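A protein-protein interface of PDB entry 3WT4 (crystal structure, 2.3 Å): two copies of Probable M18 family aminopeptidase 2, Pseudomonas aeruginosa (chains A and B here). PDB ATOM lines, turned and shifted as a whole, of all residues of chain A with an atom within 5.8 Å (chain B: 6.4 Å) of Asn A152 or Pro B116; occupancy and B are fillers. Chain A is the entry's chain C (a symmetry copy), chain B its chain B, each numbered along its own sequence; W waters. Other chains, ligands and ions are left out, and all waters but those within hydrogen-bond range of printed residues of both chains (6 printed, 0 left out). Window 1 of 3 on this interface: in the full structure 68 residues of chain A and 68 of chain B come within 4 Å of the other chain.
NH2 of Arg A120 lies within hydrogen-bond range of O of Phe B118, at 3.4 Å. The guanidinium group (NH2) of Arg A120 is in hydrogen-bond range of the backbone carbonyl oxygen (O) of Asp B119. NH2 of Arg B120 lies within hydrogen-bond range of O of Phe A118, 3.5 Å away. The backbone carbonyl oxygen (O) of Asp A119 is in hydrogen-bond range of the guanidinium group (NH2) of Arg B120 (2.9 Å). The backbone carbonyl oxygen (O) of Pro A151 sits at hydrogen-bond distance from a ring nitrogen (NE2) of His B313 (2.6 Å). The backbone carbonyl oxygen of Asn A152 sits close to a ring nitrogen (NE2) of His B313 (3.5 Å). N of Ala B399 lies close to O of Asn A152 (3.2 Å). OG of Ser B402 is in hydrogen-bond range of OD2 of Asp A119 (2.6 Å).
The backbone NH (N) of Leu B113 is in hydrogen-bond range of the backbone carbonyl oxygen (O) of His B401. The backbone carbonyl oxygen (O) of Pro B116 is in hydrogen-bond range of the guanidinium group (NE) of Arg B120, 2.9 Å away. The backbone NH of Arg B404 sits at hydrogen-bond distance from the side-chain hydroxyl of Ser B402. The backbone NH (N) of Asp A119 is in hydrogen-bond range of the backbone carbonyl oxygen (O) of Ile A150. The side-chain carboxylate of Asp A119 sits at hydrogen-bond distance from the backbone NH of Asn A152 (2.7 Å).
Among the printed residues, pairs that only touch across the chains: Asp A119 with Arg B404, Arg A120 with Arg B120, Asp A119 with Ala B399, Ala A154 with Met B400, Phe A118 with Tyr B316, Leu A153 with Tyr B316, Asn A152 with Pro B116, Pro A151 with Phe B398 and Leu A153 with Leu B113.
Of the printed residues of chain B, Leu A153 touches Leu B113 (3.9 Å) and Tyr B316 (3.7 Å). Printed residues of chain A within 4 Å of Leu B113: Leu A153 (3.9 Å). Printed residues of chain A within 4 Å of Phe B118: Arg A120 (3.4 Å). Of the printed residues of chain A, His B313 touches Pro A151 and Asn A152. Printed residues of chain A within 4 Å of Ser B402: Asp A119. The nearest residue of chain B that does not touch Asn A152 is Leu B113 (4.1 Å). The nearest printed residue of chain B that does not touch Ala A154 is Ala B399 (4.1 Å).
Of the 17 printed residues of chain B, 12 touch a printed residue of chain A. Hydrophobic or aromatic side chains of chain B within 4 Å of the printed part of chain A: Leu B113, Pro B116, His B313, Tyr B316, Phe B398, Ala B399 and Met B400. Among the printed residues, no Asp or Glu carboxylate lies within 4 Å of a Lys or Arg side-chain nitrogen of the other chain.
Phe A118 touches Arg B120, and with the chains exchanged Arg A120 touches Phe B118. Asp A119 touches Arg B120, and with the chains exchanged Arg A120 touches Asp B119. Arg B120 touches its own counterpart, Arg A120. 4 positions are printed for both chains.
Water W3 lies within hydrogen-bond range of the side-chain amide oxygen (OD1) of Asn A152, the side-chain hydroxyl (OH) of Tyr B316 and the backbone NH (N) of Leu A153. Water W5 lies within hydrogen-bond range of the backbone carbonyl oxygen (O) of Phe B118 (2.8 Å), the guanidinium group (NH2) of Arg A120 (3.0 Å) and the backbone carbonyl oxygen (O) of Ala B115 (3.3 Å). Water W1 lies within hydrogen-bond range of the backbone carbonyl oxygen of Pro A151 and a ring nitrogen (NE2) of His B313. Water W4 lies within hydrogen-bond range of the backbone carbonyl oxygen (O) of Phe A118, the guanidinium group (NH2) of Arg B120 and the backbone carbonyl oxygen (O) of Ala A115. Water W2 lies within hydrogen-bond range of the side-chain carboxylate (OD1) of Asp A119 (2.8 Å) and the backbone carbonyl oxygen (O) of Arg B404 (2.9 Å). Water W6 lies within hydrogen-bond range of N of Ala A154 and N of Ala B399.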
ATOM      1  N   ALA A 115      22.558 -15.401  -3.489  1.00  0.00           N
ATOM      2  CA  ALA A 115      22.250 -15.259  -4.904  1.00  0.00           C
ATOM      3  C   ALA A 115      23.095 -14.201  -5.634  1.00  0.00           C
ATOM      4  O   ALA A 115      23.514 -14.402  -6.779  1.00  0.00           O
ATOM      5  CB  ALA A 115      20.751 -15.018  -5.144  1.00  0.00           C
ATOM      6  N   PHE A 118      26.494 -14.774  -7.538  1.00  0.00           N
ATOM      7  CA  PHE A 118      26.523 -15.464  -8.803  1.00  0.00           C
ATOM      8  C   PHE A 118      26.645 -14.460  -9.933  1.00  0.00           C
ATOM      9  O   PHE A 118      26.067 -13.390  -9.863  1.00  0.00           O
ATOM     10  CB  PHE A 118      25.262 -16.280  -9.015  1.00  0.00           C
ATOM     11  CG  PHE A 118      25.172 -17.530  -8.191  1.00  0.00           C
ATOM     12  CD1 PHE A 118      24.881 -17.478  -6.846  1.00  0.00           C
ATOM     13  CD2 PHE A 118      25.245 -18.769  -8.780  1.00  0.00           C
ATOM     14  CE1 PHE A 118      24.682 -18.640  -6.086  1.00  0.00           C
ATOM     15  CE2 PHE A 118      25.072 -19.915  -8.020  1.00  0.00           C
ATOM     16  CZ  PHE A 118      24.742 -19.851  -6.685  1.00  0.00           C
ATOM     17  N   ASP A 119      27.359 -14.868 -10.979  1.00  0.00           N
ATOM     18  CA  ASP A 119      27.451 -14.113 -12.225  1.00  0.00           C
ATOM     19  C   ASP A 119      28.030 -12.702 -11.983  1.00  0.00           C
ATOM     20  O   ASP A 119      27.508 -11.684 -12.437  1.00  0.00           O
ATOM     21  CB  ASP A 119      26.097 -14.044 -12.899  1.00  0.00           C
ATOM     22  CG  ASP A 119      25.507 -15.383 -13.147  1.00  0.00           C
ATOM     23  OD1 ASP A 119      26.296 -16.397 -13.240  1.00  0.00           O
ATOM     24  OD2 ASP A 119      24.248 -15.405 -13.354  1.00  0.00           O
ATOM     25  N   ARG A 120      29.160 -12.704 -11.268  1.00  0.00           N
ATOM     26  CA  ARG A 120      29.943 -11.553 -10.983  1.00  0.00           C
ATOM     27  C   ARG A 120      31.393 -11.886 -11.306  1.00  0.00           C
ATOM     28  O   ARG A 120      31.798 -13.030 -11.180  1.00  0.00           O
ATOM     29  CB  ARG A 120      29.827 -11.219  -9.501  1.00  0.00           C
ATOM     30  CG  ARG A 120      28.421 -11.015  -8.995  1.00  0.00           C
ATOM     31  CD  ARG A 120      27.822  -9.646  -9.316  1.00  0.00           C
ATOM     32  NE  ARG A 120      26.486  -9.481  -8.734  1.00  0.00           N
ATOM     33  CZ  ARG A 120      25.856  -8.332  -8.571  1.00  0.00           C
ATOM     34  NH1 ARG A 120      26.368  -7.213  -9.003  1.00  0.00           N
ATOM     35  NH2 ARG A 120      24.660  -8.310  -7.996  1.00  0.00           N
ATOM     36  N   ILE A 150      31.285 -17.486 -10.204  1.00  0.00           N
ATOM     37  CA  ILE A 150      30.323 -18.457  -9.738  1.00  0.00           C
ATOM     38  C   ILE A 150      29.074 -18.398 -10.668  1.00  0.00           C
ATOM     39  O   ILE A 150      28.154 -17.623 -10.479  1.00  0.00           O
ATOM     40  CB  ILE A 150      29.915 -18.203  -8.260  1.00  0.00           C
ATOM     41  CG1 ILE A 150      31.117 -18.283  -7.343  1.00  0.00           C
ATOM     42  CG2 ILE A 150      28.870 -19.225  -7.796  1.00  0.00           C
ATOM     43  CD1 ILE A 150      30.899 -17.436  -6.113  1.00  0.00           C
ATOM     44  N   PRO A 151      29.050 -19.202 -11.710  1.00  0.00           N
ATOM     45  CA  PRO A 151      27.951 -18.995 -12.675  1.00  0.00           C
ATOM     46  C   PRO A 151      26.639 -19.586 -12.207  1.00  0.00           C
ATOM     47  O   PRO A 151      26.645 -20.680 -11.610  1.00  0.00           O
ATOM     48  CB  PRO A 151      28.413 -19.788 -13.909  1.00  0.00           C
ATOM     49  CG  PRO A 151      29.832 -20.242 -13.620  1.00  0.00           C
ATOM     50  CD  PRO A 151      29.936 -20.288 -12.124  1.00  0.00           C
ATOM     51  N   ASN A 152      25.531 -18.908 -12.532  1.00  0.00           N
ATOM     52  CA  ASN A 152      24.224 -19.504 -12.371  1.00  0.00           C
ATOM     53  C   ASN A 152      24.099 -20.699 -13.296  1.00  0.00           C
ATOM     54  O   ASN A 152      24.858 -20.820 -14.225  1.00  0.00           O
ATOM     55  CB  ASN A 152      23.093 -18.517 -12.556  1.00  0.00           C
ATOM     56  CG  ASN A 152      22.634 -17.909 -11.241  1.00  0.00           C
ATOM     57  OD1 ASN A 152      22.154 -18.591 -10.311  1.00  0.00           O
ATOM     58  ND2 ASN A 152      22.758 -16.633 -11.152  1.00  0.00           N
ATOM     59  N   LEU A 153      23.203 -21.606 -12.943  1.00  0.00           N
ATOM     60  CA  LEU A 153      22.730 -22.680 -13.819  1.00  0.00           C
ATOM     61  C   LEU A 153      21.682 -22.064 -14.711  1.00  0.00           C
ATOM     62  O   LEU A 153      20.789 -21.386 -14.214  1.00  0.00           O
ATOM     63  CB  LEU A 153      22.070 -23.814 -12.998  1.00  0.00           C
ATOM     64  CG  LEU A 153      21.478 -24.975 -13.824  1.00  0.00           C
ATOM     65  CD1 LEU A 153      22.521 -25.649 -14.726  1.00  0.00           C
ATOM     66  CD2 LEU A 153      20.771 -25.986 -12.902  1.00  0.00           C
ATOM     67  N   ALA A 154      21.761 -22.348 -16.012  1.00  0.00           N
ATOM     68  CA  ALA A 154      20.772 -21.822 -16.952  1.00  0.00           C
ATOM     69  C   ALA A 154      19.369 -22.095 -16.474  1.00  0.00           C
ATOM     70  O   ALA A 154      19.068 -23.174 -16.001  1.00  0.00           O
ATOM     71  CB  ALA A 154      20.936 -22.432 -18.354  1.00  0.00           C
ATOM     72  N   TRP A 165      14.947 -21.752  -4.656  1.00  0.00           N
ATOM     73  CA  TRP A 165      15.370 -23.062  -4.195  1.00  0.00           C
ATOM     74  C   TRP A 165      16.402 -22.777  -3.120  1.00  0.00           C
ATOM     75  O   TRP A 165      16.964 -21.711  -3.137  1.00  0.00           O
ATOM     76  CB  TRP A 165      15.966 -23.899  -5.316  1.00  0.00           C
ATOM     77  CG  TRP A 165      17.340 -23.463  -5.798  1.00  0.00           C
ATOM     78  CD1 TRP A 165      18.551 -23.995  -5.408  1.00  0.00           C
ATOM     79  CD2 TRP A 165      17.643 -22.413  -6.736  1.00  0.00           C
ATOM     80  NE1 TRP A 165      19.570 -23.346  -6.043  1.00  0.00           N
ATOM     81  CE2 TRP A 165      19.053 -22.369  -6.859  1.00  0.00           C
ATOM     82  CE3 TRP A 165      16.856 -21.494  -7.484  1.00  0.00           C
ATOM     83  CZ2 TRP A 165      19.708 -21.456  -7.724  1.00  0.00           C
ATOM     84  CZ3 TRP A 165      17.509 -20.578  -8.333  1.00  0.00           C
ATOM     85  CH2 TRP A 165      18.918 -20.558  -8.424  1.00  0.00           C
ATOM     86  N   LEU B 113      16.121 -15.121 -15.826  1.00  0.00           N
ATOM     87  CA  LEU B 113      16.424 -15.376 -14.420  1.00  0.00           C
ATOM     88  C   LEU B 113      16.268 -14.068 -13.653  1.00  0.00           C
ATOM     89  O   LEU B 113      16.950 -13.126 -13.973  1.00  0.00           O
ATOM     90  CB  LEU B 113      17.845 -15.873 -14.260  1.00  0.00           C
ATOM     91  CG  LEU B 113      18.087 -17.321 -14.637  1.00  0.00           C
ATOM     92  CD1 LEU B 113      19.565 -17.655 -14.380  1.00  0.00           C
ATOM     93  CD2 LEU B 113      17.195 -18.172 -13.779  1.00  0.00           C
ATOM     94  N   PHE B 114      15.330 -13.989 -12.713  1.00  0.00           N
ATOM     95  CA  PHE B 114      15.081 -12.741 -11.987  1.00  0.00           C
ATOM     96  C   PHE B 114      16.235 -12.355 -11.076  1.00  0.00           C
ATOM     97  O   PHE B 114      16.646 -11.179 -11.033  1.00  0.00           O
ATOM     98  CB  PHE B 114      13.773 -12.766 -11.147  1.00  0.00           C
ATOM     99  CG  PHE B 114      12.495 -13.045 -11.952  1.00  0.00           C
ATOM    100  CD1 PHE B 114      12.490 -13.030 -13.332  1.00  0.00           C
ATOM    101  CD2 PHE B 114      11.292 -13.333 -11.298  1.00  0.00           C
ATOM    102  CE1 PHE B 114      11.311 -13.294 -14.058  1.00  0.00           C
ATOM    103  CE2 PHE B 114      10.114 -13.586 -12.027  1.00  0.00           C
ATOM    104  CZ  PHE B 114      10.134 -13.596 -13.427  1.00  0.00           C
ATOM    105  N   ALA B 115      16.764 -13.314 -10.326  1.00  0.00           N
ATOM    106  CA  ALA B 115      17.614 -12.916  -9.197  1.00  0.00           C
ATOM    107  C   ALA B 115      18.859 -12.097  -9.648  1.00  0.00           C
ATOM    108  O   ALA B 115      19.259 -11.125  -9.003  1.00  0.00           O
ATOM    109  CB  ALA B 115      17.993 -14.144  -8.340  1.00  0.00           C
ATOM    110  N   PRO B 116      19.483 -12.502 -10.768  1.00  0.00           N
ATOM    111  CA  PRO B 116      20.660 -11.746 -11.185  1.00  0.00           C
ATOM    112  C   PRO B 116      20.405 -10.285 -11.571  1.00  0.00           C
ATOM    113  O   PRO B 116      21.344  -9.526 -11.640  1.00  0.00           O
ATOM    114  CB  PRO B 116      21.177 -12.522 -12.388  1.00  0.00           C
ATOM    115  CG  PRO B 116      20.536 -13.867 -12.286  1.00  0.00           C
ATOM    116  CD  PRO B 116      19.249 -13.688 -11.579  1.00  0.00           C
ATOM    117  N   TRP B 117      19.155  -9.904 -11.860  1.00  0.00           N
ATOM    118  CA  TRP B 117      18.818  -8.506 -12.128  1.00  0.00           C
ATOM    119  C   TRP B 117      18.938  -7.585 -10.937  1.00  0.00           C
ATOM    120  O   TRP B 117      19.035  -6.335 -11.080  1.00  0.00           O
ATOM    121  CB  TRP B 117      17.448  -8.406 -12.798  1.00  0.00           C
ATOM    122  CG  TRP B 117      17.571  -8.795 -14.246  1.00  0.00           C
ATOM    123  CD1 TRP B 117      17.638 -10.040 -14.737  1.00  0.00           C
ATOM    124  CD2 TRP B 117      17.769  -7.915 -15.335  1.00  0.00           C
ATOM    125  NE1 TRP B 117      17.839 -10.019 -16.064  1.00  0.00           N
ATOM    126  CE2 TRP B 117      17.960  -8.710 -16.471  1.00  0.00           C
ATOM    127  CE3 TRP B 117      17.811  -6.524 -15.461  1.00  0.00           C
ATOM    128  CZ2 TRP B 117      18.110  -8.170 -17.769  1.00  0.00           C
ATOM    129  CZ3 TRP B 117      18.020  -5.970 -16.762  1.00  0.00           C
ATOM    130  CH2 TRP B 117      18.175  -6.823 -17.892  1.00  0.00           C
ATOM    131  N   PHE B 118      18.938  -8.177  -9.737  1.00  0.00           N
ATOM    132  CA  PHE B 118      19.008  -7.358  -8.519  1.00  0.00           C
ATOM    133  C   PHE B 118      20.451  -6.920  -8.297  1.00  0.00           C
ATOM    134  O   PHE B 118      21.400  -7.678  -8.582  1.00  0.00           O
ATOM    135  CB  PHE B 118      18.550  -8.117  -7.285  1.00  0.00           C
ATOM    136  CG  PHE B 118      17.105  -8.420  -7.236  1.00  0.00           C
ATOM    137  CD1 PHE B 118      16.528  -9.276  -8.139  1.00  0.00           C
ATOM    138  CD2 PHE B 118      16.311  -7.861  -6.253  1.00  0.00           C
ATOM    139  CE1 PHE B 118      15.187  -9.595  -8.050  1.00  0.00           C
ATOM    140  CE2 PHE B 118      14.965  -8.175  -6.167  1.00  0.00           C
ATOM    141  CZ  PHE B 118      14.410  -9.083  -7.034  1.00  0.00           C
ATOM    142  N   ASP B 119      20.601  -5.722  -7.730  1.00  0.00           N
ATOM    143  CA  ASP B 119      21.899  -5.225  -7.311  1.00  0.00           C
ATOM    144  C   ASP B 119      22.915  -5.109  -8.461  1.00  0.00           C
ATOM    145  O   ASP B 119      24.099  -5.500  -8.341  1.00  0.00           O
ATOM    146  CB  ASP B 119      22.457  -6.108  -6.199  1.00  0.00           C
ATOM    147  CG  ASP B 119      21.542  -6.175  -5.029  1.00  0.00           C
ATOM    148  OD1 ASP B 119      20.703  -5.230  -4.932  1.00  0.00           O
ATOM    149  OD2 ASP B 119      21.739  -7.080  -4.201  1.00  0.00           O
ATOM    150  N   ARG B 120      22.413  -4.485  -9.534  1.00  0.00           N
ATOM    151  CA  ARG B 120      23.157  -4.175 -10.723  1.00  0.00           C
ATOM    152  C   ARG B 120      22.889  -2.736 -11.082  1.00  0.00           C
ATOM    153  O   ARG B 120      21.830  -2.241 -10.806  1.00  0.00           O
ATOM    154  CB  ARG B 120      22.673  -5.050 -11.875  1.00  0.00           C
ATOM    155  CG  ARG B 120      22.727  -6.521 -11.644  1.00  0.00           C
ATOM    156  CD  ARG B 120      24.126  -7.126 -11.756  1.00  0.00           C
ATOM    157  NE  ARG B 120      24.073  -8.563 -11.606  1.00  0.00           N
ATOM    158  CZ  ARG B 120      25.052  -9.409 -11.872  1.00  0.00           C
ATOM    159  NH1 ARG B 120      26.207  -8.993 -12.320  1.00  0.00           N
ATOM    160  NH2 ARG B 120      24.856 -10.700 -11.698  1.00  0.00           N
ATOM    161  N   HIS B 313      28.097 -27.711 -16.183  1.00  0.00           N
ATOM    162  CA  HIS B 313      28.462 -26.844 -15.080  1.00  0.00           C
ATOM    163  C   HIS B 313      28.961 -27.734 -13.940  1.00  0.00           C
ATOM    164  O   HIS B 313      28.246 -28.623 -13.452  1.00  0.00           O
ATOM    165  CB  HIS B 313      27.188 -26.073 -14.667  1.00  0.00           C
ATOM    166  CG  HIS B 313      27.400 -24.838 -13.830  1.00  0.00           C
ATOM    167  ND1 HIS B 313      28.271 -24.787 -12.768  1.00  0.00           N
ATOM    168  CD2 HIS B 313      26.799 -23.619 -13.884  1.00  0.00           C
ATOM    169  CE1 HIS B 313      28.192 -23.596 -12.202  1.00  0.00           C
ATOM    170  NE2 HIS B 313      27.320 -22.862 -12.871  1.00  0.00           N
ATOM    171  N   TYR B 316      26.781 -28.159 -10.983  1.00  0.00           N
ATOM    172  CA  TYR B 316      25.477 -28.708 -11.293  1.00  0.00           C
ATOM    173  C   TYR B 316      25.581 -29.757 -12.403  1.00  0.00           C
ATOM    174  O   TYR B 316      24.743 -29.771 -13.345  1.00  0.00           O
ATOM    175  CB  TYR B 316      24.452 -27.627 -11.783  1.00  0.00           C
ATOM    176  CG  TYR B 316      24.219 -26.439 -10.890  1.00  0.00           C
ATOM    177  CD1 TYR B 316      23.299 -26.494  -9.883  1.00  0.00           C
ATOM    178  CD2 TYR B 316      24.897 -25.234 -11.096  1.00  0.00           C
ATOM    179  CE1 TYR B 316      23.066 -25.403  -9.090  1.00  0.00           C
ATOM    180  CE2 TYR B 316      24.695 -24.149 -10.284  1.00  0.00           C
ATOM    181  CZ  TYR B 316      23.780 -24.221  -9.295  1.00  0.00           C
ATOM    182  OH  TYR B 316      23.551 -23.153  -8.455  1.00  0.00           O
ATOM    183  N   PHE B 398      27.450 -20.878 -19.814  1.00  0.00           N
ATOM    184  CA  PHE B 398      26.732 -21.052 -18.568  1.00  0.00           C
ATOM    185  C   PHE B 398      25.809 -19.874 -18.280  1.00  0.00           C
ATOM    186  O   PHE B 398      26.005 -18.749 -18.770  1.00  0.00           O
ATOM    187  CB  PHE B 398      27.702 -21.095 -17.396  1.00  0.00           C
ATOM    188  CG  PHE B 398      28.668 -22.224 -17.406  1.00  0.00           C
ATOM    189  CD1 PHE B 398      28.279 -23.520 -17.788  1.00  0.00           C
ATOM    190  CD2 PHE B 398      29.945 -22.027 -16.901  1.00  0.00           C
ATOM    191  CE1 PHE B 398      29.170 -24.552 -17.711  1.00  0.00           C
ATOM    192  CE2 PHE B 398      30.857 -23.083 -16.817  1.00  0.00           C
ATOM    193  CZ  PHE B 398      30.481 -24.350 -17.244  1.00  0.00           C
ATOM    194  N   ALA B 399      24.864 -20.124 -17.384  1.00  0.00           N
ATOM    195  CA  ALA B 399      24.056 -19.073 -16.772  1.00  0.00           C
ATOM    196  C   ALA B 399      23.146 -18.394 -17.751  1.00  0.00           C
ATOM    197  O   ALA B 399      22.813 -17.180 -17.648  1.00  0.00           O
ATOM    198  CB  ALA B 399      24.920 -18.056 -16.045  1.00  0.00           C
ATOM    199  N   MET B 400      22.672 -19.186 -18.670  1.00  0.00           N
ATOM    200  CA  MET B 400      21.914 -18.621 -19.779  1.00  0.00           C
ATOM    201  C   MET B 400      20.623 -18.013 -19.251  1.00  0.00           C
ATOM    202  O   MET B 400      19.842 -18.713 -18.515  1.00  0.00           O
ATOM    203  CB  MET B 400      21.578 -19.714 -20.807  1.00  0.00           C
ATOM    204  CG  MET B 400      21.419 -19.151 -22.229  1.00  0.00           C
ATOM    205  SD  MET B 400      21.073 -20.340 -23.545  1.00  0.00           S
ATOM    206  CE  MET B 400      22.588 -21.299 -23.577  1.00  0.00           C
ATOM    207  N   HIS B 401      20.354 -16.798 -19.723  1.00  0.00           N
ATOM    208  CA  HIS B 401      19.212 -15.942 -19.343  1.00  0.00           C
ATOM    209  C   HIS B 401      19.444 -15.183 -18.028  1.00  0.00           C
ATOM    210  O   HIS B 401      18.590 -14.431 -17.595  1.00  0.00           O
ATOM    211  CB  HIS B 401      17.863 -16.698 -19.370  1.00  0.00           C
ATOM    212  CG  HIS B 401      17.414 -17.070 -20.738  1.00  0.00           C
ATOM    213  ND1 HIS B 401      16.156 -17.564 -21.011  1.00  0.00           N
ATOM    214  CD2 HIS B 401      18.054 -17.008 -21.928  1.00  0.00           C
ATOM    215  CE1 HIS B 401      16.047 -17.785 -22.305  1.00  0.00           C
ATOM    216  NE2 HIS B 401      17.177 -17.432 -22.887  1.00  0.00           N
ATOM    217  N   SER B 402      20.666 -15.280 -17.475  1.00  0.00           N
ATOM    218  CA  SER B 402      21.094 -14.324 -16.500  1.00  0.00           C
ATOM    219  C   SER B 402      21.289 -12.942 -17.150  1.00  0.00           C
ATOM    220  O   SER B 402      21.383 -12.829 -18.359  1.00  0.00           O
ATOM    221  CB  SER B 402      22.390 -14.808 -15.812  1.00  0.00           C
ATOM    222  OG  SER B 402      22.932 -13.795 -14.929  1.00  0.00           O
ATOM    223  N   ILE B 403      21.434 -11.905 -16.321  1.00  0.00           N
ATOM    224  CA  ILE B 403      21.993 -10.640 -16.750  1.00  0.00           C
ATOM    225  C   ILE B 403      23.465 -10.691 -17.106  1.00  0.00           C
ATOM    226  O   ILE B 403      24.008  -9.731 -17.712  1.00  0.00           O
ATOM    227  CB  ILE B 403      21.717  -9.546 -15.677  1.00  0.00           C
ATOM    228  CG1 ILE B 403      21.653  -8.197 -16.303  1.00  0.00           C
ATOM    229  CG2 ILE B 403      22.709  -9.562 -14.542  1.00  0.00           C
ATOM    230  CD1 ILE B 403      21.336  -7.080 -15.339  1.00  0.00           C
ATOM    231  N   ARG B 404      24.145 -11.742 -16.685  1.00  0.00           N
ATOM    232  CA  ARG B 404      25.591 -11.868 -16.961  1.00  0.00           C
ATOM    233  C   ARG B 404      25.905 -13.332 -17.182  1.00  0.00           C
ATOM    234  O   ARG B 404      25.967 -14.118 -16.236  1.00  0.00           O
ATOM    235  CB  ARG B 404      26.445 -11.273 -15.846  1.00  0.00           C
ATOM    236  CG  ARG B 404      27.803 -10.868 -16.329  1.00  0.00           C
ATOM    237  CD  ARG B 404      28.591 -10.058 -15.318  1.00  0.00           C
ATOM    238  NE  ARG B 404      29.901  -9.599 -15.774  1.00  0.00           N
ATOM    239  CZ  ARG B 404      30.148  -8.622 -16.675  1.00  0.00           C
ATOM    240  NH1 ARG B 404      29.179  -7.979 -17.315  1.00  0.00           N
ATOM    241  NH2 ARG B 404      31.409  -8.271 -16.936  1.00  0.00           N
HETATM  242  O   HOH W   1      27.636 -22.126  -9.473  1.00  0.00           O
HETATM  243  O   HOH W   2      28.007 -16.083 -15.486  1.00  0.00           O
HETATM  244  O   HOH W   3      22.038 -21.191 -10.084  1.00  0.00           O
HETATM  245  O   HOH W   4      23.538 -12.339  -9.406  1.00  0.00           O
HETATM  246  O   HOH W   5      22.338 -10.233  -8.118  1.00  0.00           O
HETATM  247  O   HOH W   6      24.276 -23.297 -17.255  1.00  0.00           O
